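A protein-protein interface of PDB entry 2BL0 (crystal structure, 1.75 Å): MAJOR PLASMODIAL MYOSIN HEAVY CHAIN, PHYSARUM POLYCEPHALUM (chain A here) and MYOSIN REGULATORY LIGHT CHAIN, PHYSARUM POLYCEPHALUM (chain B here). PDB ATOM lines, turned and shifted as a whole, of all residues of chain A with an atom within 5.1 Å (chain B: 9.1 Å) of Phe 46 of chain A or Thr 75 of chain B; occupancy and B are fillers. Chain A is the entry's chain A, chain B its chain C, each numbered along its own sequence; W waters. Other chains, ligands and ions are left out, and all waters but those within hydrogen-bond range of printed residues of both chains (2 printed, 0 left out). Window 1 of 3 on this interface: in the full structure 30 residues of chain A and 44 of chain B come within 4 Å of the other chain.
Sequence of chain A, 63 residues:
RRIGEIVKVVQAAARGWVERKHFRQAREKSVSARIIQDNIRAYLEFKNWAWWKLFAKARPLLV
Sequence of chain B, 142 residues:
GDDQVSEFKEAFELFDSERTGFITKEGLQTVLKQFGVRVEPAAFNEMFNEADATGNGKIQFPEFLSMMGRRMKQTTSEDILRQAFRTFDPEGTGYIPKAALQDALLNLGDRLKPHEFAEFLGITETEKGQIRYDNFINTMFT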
ATOM      1  N   ASP A  38      17.721 -19.817  18.038  1.00  0.00           N
ATOM      2  CA  ASP A  38      17.450 -19.187  19.325  1.00  0.00           C
ATOM      3  C   ASP A  38      18.314 -19.850  20.390  1.00  0.00           C
ATOM      4  O   ASP A  38      18.876 -19.176  21.247  1.00  0.00           O
ATOM      5  CB  ASP A  38      15.990 -19.371  19.729  1.00  0.00           C
ATOM      6  CG  ASP A  38      15.020 -18.490  18.942  1.00  0.00           C
ATOM      7  OD1 ASP A  38      15.452 -17.573  18.235  1.00  0.00           O
ATOM      8  OD2 ASP A  38      13.794 -18.661  19.028  1.00  0.00           O
ATOM      9  N   ASN A  39      18.418 -21.174  20.315  1.00  0.00           N
ATOM     10  CA  ASN A  39      19.237 -21.921  21.257  1.00  0.00           C
ATOM     11  C   ASN A  39      20.729 -21.669  21.095  1.00  0.00           C
ATOM     12  O   ASN A  39      21.429 -21.512  22.087  1.00  0.00           O
ATOM     13  CB  ASN A  39      18.918 -23.419  21.177  1.00  0.00           C
ATOM     14  CG  ASN A  39      17.715 -23.778  21.981  1.00  0.00           C
ATOM     15  OD1 ASN A  39      17.745 -23.707  23.231  1.00  0.00           O
ATOM     16  ND2 ASN A  39      16.611 -24.133  21.300  1.00  0.00           N
ATOM     17  N   ALA A  42      21.521 -17.962  22.257  1.00  0.00           N
ATOM     18  CA  ALA A  42      21.445 -17.857  23.714  1.00  0.00           C
ATOM     19  C   ALA A  42      22.670 -18.469  24.373  1.00  0.00           C
ATOM     20  O   ALA A  42      23.312 -17.838  25.204  1.00  0.00           O
ATOM     21  CB  ALA A  42      20.200 -18.519  24.222  1.00  0.00           C
ATOM     22  N   TYR A  43      22.987 -19.696  23.981  1.00  0.00           N
ATOM     23  CA  TYR A  43      24.146 -20.386  24.502  1.00  0.00           C
ATOM     24  C   TYR A  43      25.435 -19.587  24.309  1.00  0.00           C
ATOM     25  O   TYR A  43      26.253 -19.476  25.220  1.00  0.00           O
ATOM     26  CB  TYR A  43      24.253 -21.767  23.842  1.00  0.00           C
ATOM     27  CG  TYR A  43      25.414 -22.589  24.341  1.00  0.00           C
ATOM     28  CD1 TYR A  43      25.348 -23.261  25.553  1.00  0.00           C
ATOM     29  CD2 TYR A  43      26.593 -22.673  23.606  1.00  0.00           C
ATOM     30  CE1 TYR A  43      26.425 -24.010  26.010  1.00  0.00           C
ATOM     31  CE2 TYR A  43      27.661 -23.413  24.054  1.00  0.00           C
ATOM     32  CZ  TYR A  43      27.577 -24.080  25.244  1.00  0.00           C
ATOM     33  OH  TYR A  43      28.663 -24.804  25.676  1.00  0.00           O
ATOM     34  N   LEU A  44      25.642 -19.037  23.112  1.00  0.00           N
ATOM     35  CA  LEU A  44      26.867 -18.295  22.869  1.00  0.00           C
ATOM     36  C   LEU A  44      26.942 -17.038  23.739  1.00  0.00           C
ATOM     37  O   LEU A  44      28.031 -16.584  24.070  1.00  0.00           O
ATOM     38  CB  LEU A  44      27.002 -17.930  21.391  1.00  0.00           C
ATOM     39  CG  LEU A  44      27.162 -19.145  20.477  1.00  0.00           C
ATOM     40  CD1 LEU A  44      27.095 -18.705  19.042  1.00  0.00           C
ATOM     41  CD2 LEU A  44      28.475 -19.898  20.753  1.00  0.00           C
ATOM     42  N   GLU A  45      25.779 -16.507  24.114  1.00  0.00           N
ATOM     43  CA  GLU A  45      25.673 -15.332  24.980  1.00  0.00           C
ATOM     44  C   GLU A  45      25.886 -15.649  26.453  1.00  0.00           C
ATOM     45  O   GLU A  45      26.420 -14.811  27.178  1.00  0.00           O
ATOM     46  CB  GLU A  45      24.315 -14.623  24.803  1.00  0.00           C
ATOM     47  CG  GLU A  45      24.189 -13.842  23.497  1.00  0.00           C
ATOM     48  CD  GLU A  45      22.750 -13.436  23.156  1.00  0.00           C
ATOM     49  OE1 GLU A  45      21.879 -13.426  24.064  1.00  0.00           O
ATOM     50  OE2 GLU A  45      22.484 -13.124  21.966  1.00  0.00           O
ATOM     51  N   PHE A  46      25.529 -16.847  26.907  1.00  0.00           N
ATOM     52  CA  PHE A  46      25.655 -17.159  28.320  1.00  0.00           C
ATOM     53  C   PHE A  46      26.686 -18.248  28.683  1.00  0.00           C
ATOM     54  O   PHE A  46      26.805 -18.593  29.841  1.00  0.00           O
ATOM     55  CB  PHE A  46      24.274 -17.457  28.963  1.00  0.00           C
ATOM     56  CG  PHE A  46      23.579 -18.723  28.469  1.00  0.00           C
ATOM     57  CD1 PHE A  46      24.162 -19.977  28.570  1.00  0.00           C
ATOM     58  CD2 PHE A  46      22.286 -18.647  27.974  1.00  0.00           C
ATOM     59  CE1 PHE A  46      23.493 -21.120  28.149  1.00  0.00           C
ATOM     60  CE2 PHE A  46      21.608 -19.788  27.560  1.00  0.00           C
ATOM     61  CZ  PHE A  46      22.210 -21.017  27.640  1.00  0.00           C
ATOM     62  N   LYS A  47      27.433 -18.789  27.717  1.00  0.00           N
ATOM     63  CA  LYS A  47      28.249 -19.986  27.990  1.00  0.00           C
ATOM     64  C   LYS A  47      29.315 -19.794  29.054  1.00  0.00           C
ATOM     65  O   LYS A  47      29.733 -20.752  29.699  1.00  0.00           O
ATOM     66  CB  LYS A  47      28.907 -20.520  26.723  1.00  0.00           C
ATOM     67  CG  LYS A  47      29.905 -19.605  26.049  1.00  0.00           C
ATOM     68  CD  LYS A  47      30.321 -20.286  24.750  1.00  0.00           C
ATOM     69  CE  LYS A  47      31.345 -19.527  23.947  1.00  0.00           C
ATOM     70  NZ  LYS A  47      31.622 -20.310  22.709  1.00  0.00           N
ATOM     71  N   ASN A  48      29.728 -18.564  29.260  1.00  0.00           N
ATOM     72  CA  ASN A  48      30.774 -18.276  30.227  1.00  0.00           C
ATOM     73  C   ASN A  48      30.235 -17.520  31.425  1.00  0.00           C
ATOM     74  O   ASN A  48      30.990 -17.092  32.293  1.00  0.00           O
ATOM     75  CB  ASN A  48      31.935 -17.554  29.547  1.00  0.00           C
ATOM     76  CG  ASN A  48      32.652 -18.451  28.542  1.00  0.00           C
ATOM     77  OD1 ASN A  48      32.881 -18.072  27.396  1.00  0.00           O
ATOM     78  ND2 ASN A  48      32.997 -19.669  28.977  1.00  0.00           N
ATOM     79  N   TRP A  49      28.911 -17.442  31.506  1.00  0.00           N
ATOM     80  CA  TRP A  49      28.228 -16.776  32.604  1.00  0.00           C
ATOM     81  C   TRP A  49      28.207 -17.659  33.827  1.00  0.00           C
ATOM     82  O   TRP A  49      27.785 -18.802  33.746  1.00  0.00           O
ATOM     83  CB  TRP A  49      26.787 -16.534  32.192  1.00  0.00           C
ATOM     84  CG  TRP A  49      25.971 -15.712  33.112  1.00  0.00           C
ATOM     85  CD1 TRP A  49      26.386 -14.651  33.855  1.00  0.00           C
ATOM     86  CD2 TRP A  49      24.560 -15.831  33.337  1.00  0.00           C
ATOM     87  NE1 TRP A  49      25.326 -14.104  34.534  1.00  0.00           N
ATOM     88  CE2 TRP A  49      24.188 -14.807  34.227  1.00  0.00           C
ATOM     89  CE3 TRP A  49      23.567 -16.713  32.883  1.00  0.00           C
ATOM     90  CZ2 TRP A  49      22.868 -14.641  34.673  1.00  0.00           C
ATOM     91  CZ3 TRP A  49      22.258 -16.535  33.322  1.00  0.00           C
ATOM     92  CH2 TRP A  49      21.921 -15.514  34.191  1.00  0.00           C
ATOM     93  N   TRP A  52      24.936 -19.506  34.595  1.00  0.00           N
ATOM     94  CA  TRP A  52      24.774 -20.637  33.690  1.00  0.00           C
ATOM     95  C   TRP A  52      25.556 -21.855  34.139  1.00  0.00           C
ATOM     96  O   TRP A  52      25.021 -22.956  34.128  1.00  0.00           O
ATOM     97  CB  TRP A  52      25.209 -20.275  32.273  1.00  0.00           C
ATOM     98  CG  TRP A  52      25.516 -21.482  31.431  1.00  0.00           C
ATOM     99  CD1 TRP A  52      26.731 -21.867  30.954  1.00  0.00           C
ATOM    100  CD2 TRP A  52      24.583 -22.451  30.989  1.00  0.00           C
ATOM    101  NE1 TRP A  52      26.612 -23.032  30.232  1.00  0.00           N
ATOM    102  CE2 TRP A  52      25.294 -23.412  30.239  1.00  0.00           C
ATOM    103  CE3 TRP A  52      23.199 -22.608  31.140  1.00  0.00           C
ATOM    104  CZ2 TRP A  52      24.672 -24.506  29.648  1.00  0.00           C
ATOM    105  CZ3 TRP A  52      22.583 -23.687  30.553  1.00  0.00           C
ATOM    106  CH2 TRP A  52      23.315 -24.622  29.815  1.00  0.00           C
ATOM    107  N   ASP B   2       4.278 -22.760  32.867  1.00  0.00           N
ATOM    108  CA  ASP B   2       5.508 -22.760  32.051  1.00  0.00           C
ATOM    109  C   ASP B   2       6.617 -23.672  32.625  1.00  0.00           C
ATOM    110  O   ASP B   2       6.923 -23.627  33.826  1.00  0.00           O
ATOM    111  CB  ASP B   2       6.046 -21.335  31.877  1.00  0.00           C
ATOM    112  CG  ASP B   2       7.258 -21.274  30.986  1.00  0.00           C
ATOM    113  OD1 ASP B   2       8.373 -21.190  31.529  1.00  0.00           O
ATOM    114  OD2 ASP B   2       7.195 -21.283  29.740  1.00  0.00           O
ATOM    115  N   ASP B   3       7.223 -24.474  31.746  1.00  0.00           N
ATOM    116  CA  ASP B   3       8.255 -25.446  32.131  1.00  0.00           C
ATOM    117  C   ASP B   3       9.613 -24.819  32.494  1.00  0.00           C
ATOM    118  O   ASP B   3      10.347 -25.360  33.324  1.00  0.00           O
ATOM    119  CB  ASP B   3       8.474 -26.474  31.011  1.00  0.00           C
ATOM    120  CG  ASP B   3       7.278 -27.404  30.811  1.00  0.00           C
ATOM    121  OD1 ASP B   3       6.385 -27.452  31.685  1.00  0.00           O
ATOM    122  OD2 ASP B   3       7.150 -28.133  29.801  1.00  0.00           O
ATOM    123  N   GLN B   4       9.960 -23.725  31.826  1.00  0.00           N
ATOM    124  CA  GLN B   4      11.165 -22.957  32.140  1.00  0.00           C
ATOM    125  C   GLN B   4      11.126 -22.465  33.582  1.00  0.00           C
ATOM    126  O   GLN B   4      12.080 -22.648  34.327  1.00  0.00           O
ATOM    127  CB  GLN B   4      11.285 -21.752  31.195  1.00  0.00           C
ATOM    128  CG  GLN B   4      12.645 -21.544  30.555  1.00  0.00           C
ATOM    129  CD  GLN B   4      12.527 -21.045  29.115  1.00  0.00           C
ATOM    130  OE1 GLN B   4      13.069 -21.661  28.190  1.00  0.00           O
ATOM    131  NE2 GLN B   4      11.800 -19.937  28.922  1.00  0.00           N
ATOM    132  N   GLU B   7      11.570 -25.188  36.191  1.00  0.00           N
ATOM    133  CA  GLU B   7      12.953 -25.599  36.237  1.00  0.00           C
ATOM    134  C   GLU B   7      13.801 -24.561  37.002  1.00  0.00           C
ATOM    135  O   GLU B   7      14.672 -24.907  37.807  1.00  0.00           O
ATOM    136  CB  GLU B   7      13.484 -25.756  34.823  1.00  0.00           C
ATOM    137  CG  GLU B   7      14.876 -26.314  34.777  1.00  0.00           C
ATOM    138  CD  GLU B   7      15.294 -26.722  33.391  1.00  0.00           C
ATOM    139  OE1 GLU B   7      15.319 -25.846  32.490  1.00  0.00           O
ATOM    140  OE2 GLU B   7      15.615 -27.910  33.217  1.00  0.00           O
ATOM    141  N   PHE B   8      13.558 -23.285  36.743  1.00  0.00           N
ATOM    142  CA  PHE B   8      14.304 -22.268  37.481  1.00  0.00           C
ATOM    143  C   PHE B   8      13.952 -22.297  38.952  1.00  0.00           C
ATOM    144  O   PHE B   8      14.813 -22.092  39.782  1.00  0.00           O
ATOM    145  CB  PHE B   8      14.095 -20.868  36.910  1.00  0.00           C
ATOM    146  CG  PHE B   8      14.700 -20.676  35.556  1.00  0.00           C
ATOM    147  CD1 PHE B   8      15.935 -21.239  35.235  1.00  0.00           C
ATOM    148  CD2 PHE B   8      14.027 -19.951  34.586  1.00  0.00           C
ATOM    149  CE1 PHE B   8      16.478 -21.060  33.982  1.00  0.00           C
ATOM    150  CE2 PHE B   8      14.575 -19.777  33.352  1.00  0.00           C
ATOM    151  CZ  PHE B   8      15.807 -20.338  33.054  1.00  0.00           C
ATOM    152  N   MET B  67      16.264 -12.673  36.310  1.00  0.00           N
ATOM    153  CA  MET B  67      17.625 -12.673  35.775  1.00  0.00           C
ATOM    154  C   MET B  67      17.853 -13.838  34.820  1.00  0.00           C
ATOM    155  O   MET B  67      18.353 -13.638  33.689  1.00  0.00           O
ATOM    156  CB  MET B  67      18.649 -12.683  36.915  1.00  0.00           C
ATOM    157  CG  MET B  67      20.104 -12.859  36.451  1.00  0.00           C
ATOM    158  SD  MET B  67      21.160 -13.302  37.784  1.00  0.00           S
ATOM    159  CE  MET B  67      20.668 -14.984  38.073  1.00  0.00           C
ATOM    160  N   MET B  68      17.463 -15.038  35.250  1.00  0.00           N
ATOM    161  CA  MET B  68      17.659 -16.237  34.445  1.00  0.00           C
ATOM    162  C   MET B  68      16.822 -16.144  33.165  1.00  0.00           C
ATOM    163  O   MET B  68      17.301 -16.484  32.086  1.00  0.00           O
ATOM    164  CB  MET B  68      17.293 -17.496  35.224  1.00  0.00           C
ATOM    165  CG  MET B  68      18.175 -17.783  36.432  1.00  0.00           C
ATOM    166  SD  MET B  68      19.879 -18.103  35.973  1.00  0.00           S
ATOM    167  CE  MET B  68      19.769 -19.598  35.166  1.00  0.00           C
ATOM    168  N   GLY B  69      15.575 -15.692  33.310  1.00  0.00           N
ATOM    169  CA  GLY B  69      14.691 -15.435  32.172  1.00  0.00           C
ATOM    170  C   GLY B  69      15.253 -14.484  31.135  1.00  0.00           C
ATOM    171  O   GLY B  69      15.137 -14.739  29.929  1.00  0.00           O
ATOM    172  N   ARG B  70      15.880 -13.400  31.591  1.00  0.00           N
ATOM    173  CA  ARG B  70      16.472 -12.409  30.697  1.00  0.00           C
ATOM    174  C   ARG B  70      17.525 -13.080  29.807  1.00  0.00           C
ATOM    175  O   ARG B  70      17.536 -12.882  28.596  1.00  0.00           O
ATOM    176  CB  ARG B  70      17.102 -11.250  31.493  1.00  0.00           C
ATOM    177  CG  ARG B  70      16.097 -10.173  32.000  1.00  0.00           C
ATOM    178  CD  ARG B  70      16.705  -9.032  32.889  1.00  0.00           C
ATOM    179  NE  ARG B  70      17.832  -9.460  33.740  1.00  0.00           N
ATOM    180  CZ  ARG B  70      19.117  -9.545  33.344  1.00  0.00           C
ATOM    181  NH1 ARG B  70      19.483  -9.230  32.102  1.00  0.00           N
ATOM    182  NH2 ARG B  70      20.048  -9.956  34.196  1.00  0.00           N
ATOM    183  N   ARG B  71      18.358 -13.926  30.397  1.00  0.00           N
ATOM    184  CA  ARG B  71      19.462 -14.529  29.668  1.00  0.00           C
ATOM    185  C   ARG B  71      19.060 -15.797  28.916  1.00  0.00           C
ATOM    186  O   ARG B  71      19.706 -16.145  27.929  1.00  0.00           O
ATOM    187  CB  ARG B  71      20.639 -14.819  30.619  1.00  0.00           C
ATOM    188  CG  ARG B  71      21.190 -13.607  31.351  1.00  0.00           C
ATOM    189  CD  ARG B  71      21.985 -12.629  30.478  1.00  0.00           C
ATOM    190  NE  ARG B  71      23.236 -13.199  29.959  1.00  0.00           N
ATOM    191  CZ  ARG B  71      24.435 -13.124  30.550  1.00  0.00           C
ATOM    192  NH1 ARG B  71      25.483 -13.695  29.971  1.00  0.00           N
ATOM    193  NH2 ARG B  71      24.604 -12.496  31.713  1.00  0.00           N
ATOM    194  N   MET B  72      18.004 -16.486  29.364  1.00  0.00           N
ATOM    195  CA  MET B  72      17.684 -17.825  28.859  1.00  0.00           C
ATOM    196  C   MET B  72      16.283 -17.993  28.251  1.00  0.00           C
ATOM    197  O   MET B  72      15.876 -19.119  27.929  1.00  0.00           O
ATOM    198  CB  MET B  72      17.849 -18.848  29.980  1.00  0.00           C
ATOM    199  CG  MET B  72      19.265 -18.986  30.468  1.00  0.00           C
ATOM    200  SD  MET B  72      19.466 -20.439  31.560  1.00  0.00           S
ATOM    201  CE  MET B  72      19.055 -21.747  30.492  1.00  0.00           C
ATOM    202  N   LYS B  73      15.552 -16.897  28.084  1.00  0.00           N
ATOM    203  CA  LYS B  73      14.123 -16.994  27.741  1.00  0.00           C
ATOM    204  C   LYS B  73      13.864 -17.605  26.370  1.00  0.00           C
ATOM    205  O   LYS B  73      12.824 -18.230  26.169  1.00  0.00           O
ATOM    206  CB  LYS B  73      13.404 -15.646  27.829  1.00  0.00           C
ATOM    207  CG  LYS B  73      14.077 -14.471  27.085  1.00  0.00           C
ATOM    208  CD  LYS B  73      13.142 -13.258  26.966  1.00  0.00           C
ATOM    209  CE  LYS B  73      13.715 -12.158  26.057  1.00  0.00           C
ATOM    210  NZ  LYS B  73      14.844 -12.598  25.174  1.00  0.00           N
ATOM    211  N   GLN B  74      14.789 -17.420  25.437  1.00  0.00           N
ATOM    212  CA  GLN B  74      14.629 -17.974  24.093  1.00  0.00           C
ATOM    213  C   GLN B  74      15.142 -19.400  23.938  1.00  0.00           C
ATOM    214  O   GLN B  74      14.951 -20.008  22.891  1.00  0.00           O
ATOM    215  CB  GLN B  74      15.287 -17.060  23.068  1.00  0.00           C
ATOM    216  CG  GLN B  74      14.795 -15.615  23.143  1.00  0.00           C
ATOM    217  CD  GLN B  74      13.280 -15.506  23.318  1.00  0.00           C
ATOM    218  OE1 GLN B  74      12.512 -16.177  22.625  1.00  0.00           O
ATOM    219  NE2 GLN B  74      12.854 -14.649  24.230  1.00  0.00           N
ATOM    220  N   THR B  75      15.759 -19.959  24.981  1.00  0.00           N
ATOM    221  CA  THR B  75      16.081 -21.382  24.931  1.00  0.00           C
ATOM    222  C   THR B  75      14.803 -22.201  25.030  1.00  0.00           C
ATOM    223  O   THR B  75      13.757 -21.698  25.460  1.00  0.00           O
ATOM    224  CB  THR B  75      17.023 -21.825  26.070  1.00  0.00           C
ATOM    225  OG1 THR B  75      16.370 -21.645  27.338  1.00  0.00           O
ATOM    226  CG2 THR B  75      18.277 -20.967  26.103  1.00  0.00           C
ATOM    227  N   THR B  76      14.903 -23.470  24.650  1.00  0.00           N
ATOM    228  CA  THR B  76      13.804 -24.412  24.787  1.00  0.00           C
ATOM    229  C   THR B  76      14.265 -25.641  25.561  1.00  0.00           C
ATOM    230  O   THR B  76      15.445 -25.774  25.914  1.00  0.00           O
ATOM    231  CB  THR B  76      13.295 -24.870  23.381  1.00  0.00           C
ATOM    232  OG1 THR B  76      14.350 -25.565  22.690  1.00  0.00           O
ATOM    233  CG2 THR B  76      12.918 -23.688  22.494  1.00  0.00           C
ATOM    234  N   SER B  77      13.329 -26.543  25.809  1.00  0.00           N
ATOM    235  CA  SER B  77      13.652 -27.842  26.410  1.00  0.00           C
ATOM    236  C   SER B  77      14.546 -28.662  25.477  1.00  0.00           C
ATOM    237  O   SER B  77      14.676 -28.362  24.273  1.00  0.00           O
ATOM    238  CB  SER B  77      12.392 -28.642  26.760  1.00  0.00           C
ATOM    239  OG  SER B  77      11.290 -28.283  25.941  1.00  0.00           O
ATOM    240  N   GLU B  78      15.175 -29.692  26.042  1.00  0.00           N
ATOM    241  CA  GLU B  78      16.080 -30.537  25.270  1.00  0.00           C
ATOM    242  C   GLU B  78      15.337 -31.232  24.143  1.00  0.00           C
ATOM    243  O   GLU B  78      15.866 -31.358  23.041  1.00  0.00           O
ATOM    244  CB  GLU B  78      16.736 -31.587  26.158  1.00  0.00           C
ATOM    245  CG  GLU B  78      17.922 -32.296  25.511  1.00  0.00           C
ATOM    246  CD  GLU B  78      18.532 -33.354  26.408  1.00  0.00           C
ATOM    247  OE1 GLU B  78      18.314 -33.293  27.637  1.00  0.00           O
ATOM    248  OE2 GLU B  78      19.226 -34.253  25.884  1.00  0.00           O
ATOM    249  N   ILE B  80      12.598 -30.260  22.553  1.00  0.00           N
ATOM    250  CA  ILE B  80      12.169 -29.376  21.478  1.00  0.00           C
ATOM    251  C   ILE B  80      13.339 -29.080  20.549  1.00  0.00           C
ATOM    252  O   ILE B  80      13.158 -29.022  19.332  1.00  0.00           O
ATOM    253  CB  ILE B  80      11.486 -28.103  22.033  1.00  0.00           C
ATOM    254  CG1 ILE B  80      10.047 -28.455  22.437  1.00  0.00           C
ATOM    255  CG2 ILE B  80      11.467 -26.978  20.988  1.00  0.00           C
ATOM    256  CD1 ILE B  80       9.348 -27.423  23.261  1.00  0.00           C
ATOM    257  N   LEU B  81      14.530 -28.910  21.117  1.00  0.00           N
ATOM    258  CA  LEU B  81      15.737 -28.674  20.329  1.00  0.00           C
ATOM    259  C   LEU B  81      16.119 -29.920  19.526  1.00  0.00           C
ATOM    260  O   LEU B  81      16.523 -29.822  18.362  1.00  0.00           O
ATOM    261  CB  LEU B  81      16.887 -28.224  21.238  1.00  0.00           C
ATOM    262  CG  LEU B  81      18.263 -28.009  20.598  1.00  0.00           C
ATOM    263  CD1 LEU B  81      18.202 -27.038  19.419  1.00  0.00           C
ATOM    264  CD2 LEU B  81      19.285 -27.529  21.620  1.00  0.00           C
ATOM    265  N   PHE B 136      26.488 -30.112  20.428  1.00  0.00           N
ATOM    266  CA  PHE B 136      25.886 -28.852  20.891  1.00  0.00           C
ATOM    267  C   PHE B 136      24.852 -29.063  22.000  1.00  0.00           C
ATOM    268  O   PHE B 136      24.890 -28.387  23.034  1.00  0.00           O
ATOM    269  CB  PHE B 136      25.233 -28.078  19.741  1.00  0.00           C
ATOM    270  CG  PHE B 136      24.413 -26.899  20.213  1.00  0.00           C
ATOM    271  CD1 PHE B 136      23.044 -26.845  19.996  1.00  0.00           C
ATOM    272  CD2 PHE B 136      25.015 -25.863  20.914  1.00  0.00           C
ATOM    273  CE1 PHE B 136      22.298 -25.761  20.435  1.00  0.00           C
ATOM    274  CE2 PHE B 136      24.272 -24.785  21.369  1.00  0.00           C
ATOM    275  CZ  PHE B 136      22.912 -24.735  21.133  1.00  0.00           C
ATOM    276  N   THR B 139      26.003 -30.009  25.491  1.00  0.00           N
ATOM    277  CA  THR B 139      26.660 -28.922  26.225  1.00  0.00           C
ATOM    278  C   THR B 139      25.679 -28.096  27.056  1.00  0.00           C
ATOM    279  O   THR B 139      26.094 -27.297  27.893  1.00  0.00           O
ATOM    280  CB  THR B 139      27.474 -27.996  25.298  1.00  0.00           C
ATOM    281  OG1 THR B 139      27.959 -28.726  24.172  1.00  0.00           O
ATOM    282  CG2 THR B 139      28.760 -27.565  26.001  1.00  0.00           C
ATOM    283  N   MET B 140      24.387 -28.299  26.824  1.00  0.00           N
ATOM    284  CA  MET B 140      23.340 -27.589  27.546  1.00  0.00           C
ATOM    285  C   MET B 140      22.562 -28.494  28.502  1.00  0.00           C
ATOM    286  O   MET B 140      22.079 -28.031  29.537  1.00  0.00           O
ATOM    287  CB  MET B 140      22.399 -26.912  26.541  1.00  0.00           C
ATOM    288  CG  MET B 140      22.423 -25.413  26.654  1.00  0.00           C
ATOM    289  SD  MET B 140      21.868 -24.485  25.251  1.00  0.00           S
ATOM    290  CE  MET B 140      20.822 -25.610  24.344  1.00  0.00           C
ATOM    291  N   PHE B 141      22.453 -29.777  28.163  1.00  0.00           N
ATOM    292  CA  PHE B 141      21.814 -30.764  29.028  1.00  0.00           C
ATOM    293  C   PHE B 141      22.753 -31.962  29.229  1.00  0.00           C
ATOM    294  O   PHE B 141      22.586 -33.008  28.591  1.00  0.00           O
ATOM    295  CB  PHE B 141      20.477 -31.222  28.426  1.00  0.00           C
ATOM    296  CG  PHE B 141      19.625 -30.102  27.895  1.00  0.00           C
ATOM    297  CD1 PHE B 141      19.885 -29.550  26.649  1.00  0.00           C
ATOM    298  CD2 PHE B 141      18.557 -29.607  28.633  1.00  0.00           C
ATOM    299  CE1 PHE B 141      19.107 -28.521  26.147  1.00  0.00           C
ATOM    300  CE2 PHE B 141      17.772 -28.574  28.126  1.00  0.00           C
ATOM    301  CZ  PHE B 141      18.051 -28.036  26.883  1.00  0.00           C
HETATM  302  O   HOH W   1      13.719 -15.434  20.008  1.00  0.00           O
HETATM  303  O   HOH W   2      12.764 -20.575  21.142  1.00  0.00           O
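O of Glu 45 of chain A lies within hydrogen-bond range of NH1 of Arg 71 of chain B, at 3.2 Å.
OG1 of Thr 76 of chain B lies within hydrogen-bond range of ND2 of Asn 39 of chain A, 3.0 Å away.
The guanidinium group (NH2) of Arg 71 of chain B lies close to the indole nitrogen (NE1) of Trp 49 of chain A, 3.3 Å away.
The backbone carbonyl oxygen (O) of Met 72 of chain B sits at hydrogen-bond distance from the side-chain hydroxyl (OG1) of Thr 75 of chain B (2.6 Å).
O of Thr 75 of chain B lies close to OE1 of Gln 4 of chain B (2.8 Å).
The side-chain amino group (NZ) of Lys 73 of chain B sits close to the side-chain amide nitrogen (NE2) of Gln 74 of chain B, 3.0 Å away.
The side-chain hydroxyl (OG1) of Thr 139 of chain B is in hydrogen-bond range of the backbone carbonyl oxygen (O) of Phe 136 of chain B (3.3 Å).
Asp 38 of chain A touches Gln 74 of chain B (CB to O, 3.4 Å).
CA of Thr 75 of chain B touches OD1 of Asn 39 of chain A (3.3 Å).
Asn 39 of chain A touches Leu 81 of chain B.
Asn 39 of chain A touches Phe 136 of chain B.
OD1 of Asn 39 of chain A touches CE of Met 140 of chain B (3.8 Å).
Thr 75 of chain B touches Ala 42 of chain A (CG2 to CB, 3.6 Å).
Phe 136 of chain B touches Tyr 43 of chain A.
Met 140 of chain B touches Tyr 43 of chain A.
Thr 75 of chain B touches Phe 46 of chain A (CG2 to CE2, 3.8 Å).
Phe 46 of chain A touches just these residues of chain B: Arg 71, Met 72 and Thr 75.
Of chain A, only Asn 39 (3.3 Å), Ala 42 (3.6 Å) and Phe 46 (3.8 Å) come within 4 Å of Thr 75 of chain B.
Of the printed residues of chain B, Trp 49 of chain A touches Met 67, Met 68 and Arg 71.
Printed residues of chain A within 4 Å of Met 67 of chain B: Trp 49.
Of the printed residues of chain A, Phe 136 of chain B touches Asn 39 (3.7 Å) and Tyr 43 (3.9 Å).
Of the printed residues of chain B, Trp 52 of chain A touches Thr 139 (3.6 Å) and Met 140 (3.4 Å).
Of the printed residues of chain B, Asn 39 of chain A touches Thr 75, Thr 76, Leu 81, Phe 136 and Met 140.
The nearest residue of chain B that does not touch Phe 46 of chain A is Met 140 of chain B (4.2 Å).
The nearest residue of chain A that does not touch Thr 75 of chain B is Asp 38 of chain A (4.9 Å).
The nearest printed residue of chain A that does not touch Thr 139 of chain B is Phe 46 of chain A (6.7 Å).
Of the 23 printed residues of chain B, 11 touch a printed residue of chain A.
Hydrophobic or aromatic side chains of chain B within 4 Å of the printed part of chain A: Met 67, Met 68, Met 72, Leu 81, Phe 136 and Met 140.
Of the 11 printed residues of chain A, 8 touch a printed residue of chain B.
Among the printed residues, 19 pairs touch across the chains.
Water W2 lies within hydrogen-bond range of O of Gln 74 of chain B (2.9 Å) and OD2 of Asp 38 of chain A (3.0 Å).
Water W1 bridges the side-chain amide oxygen (OE1) of Gln 74 of chain B (3.0 Å) and the side-chain carboxylate (OD1) of Asp 38 of chain A (3.3 Å).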
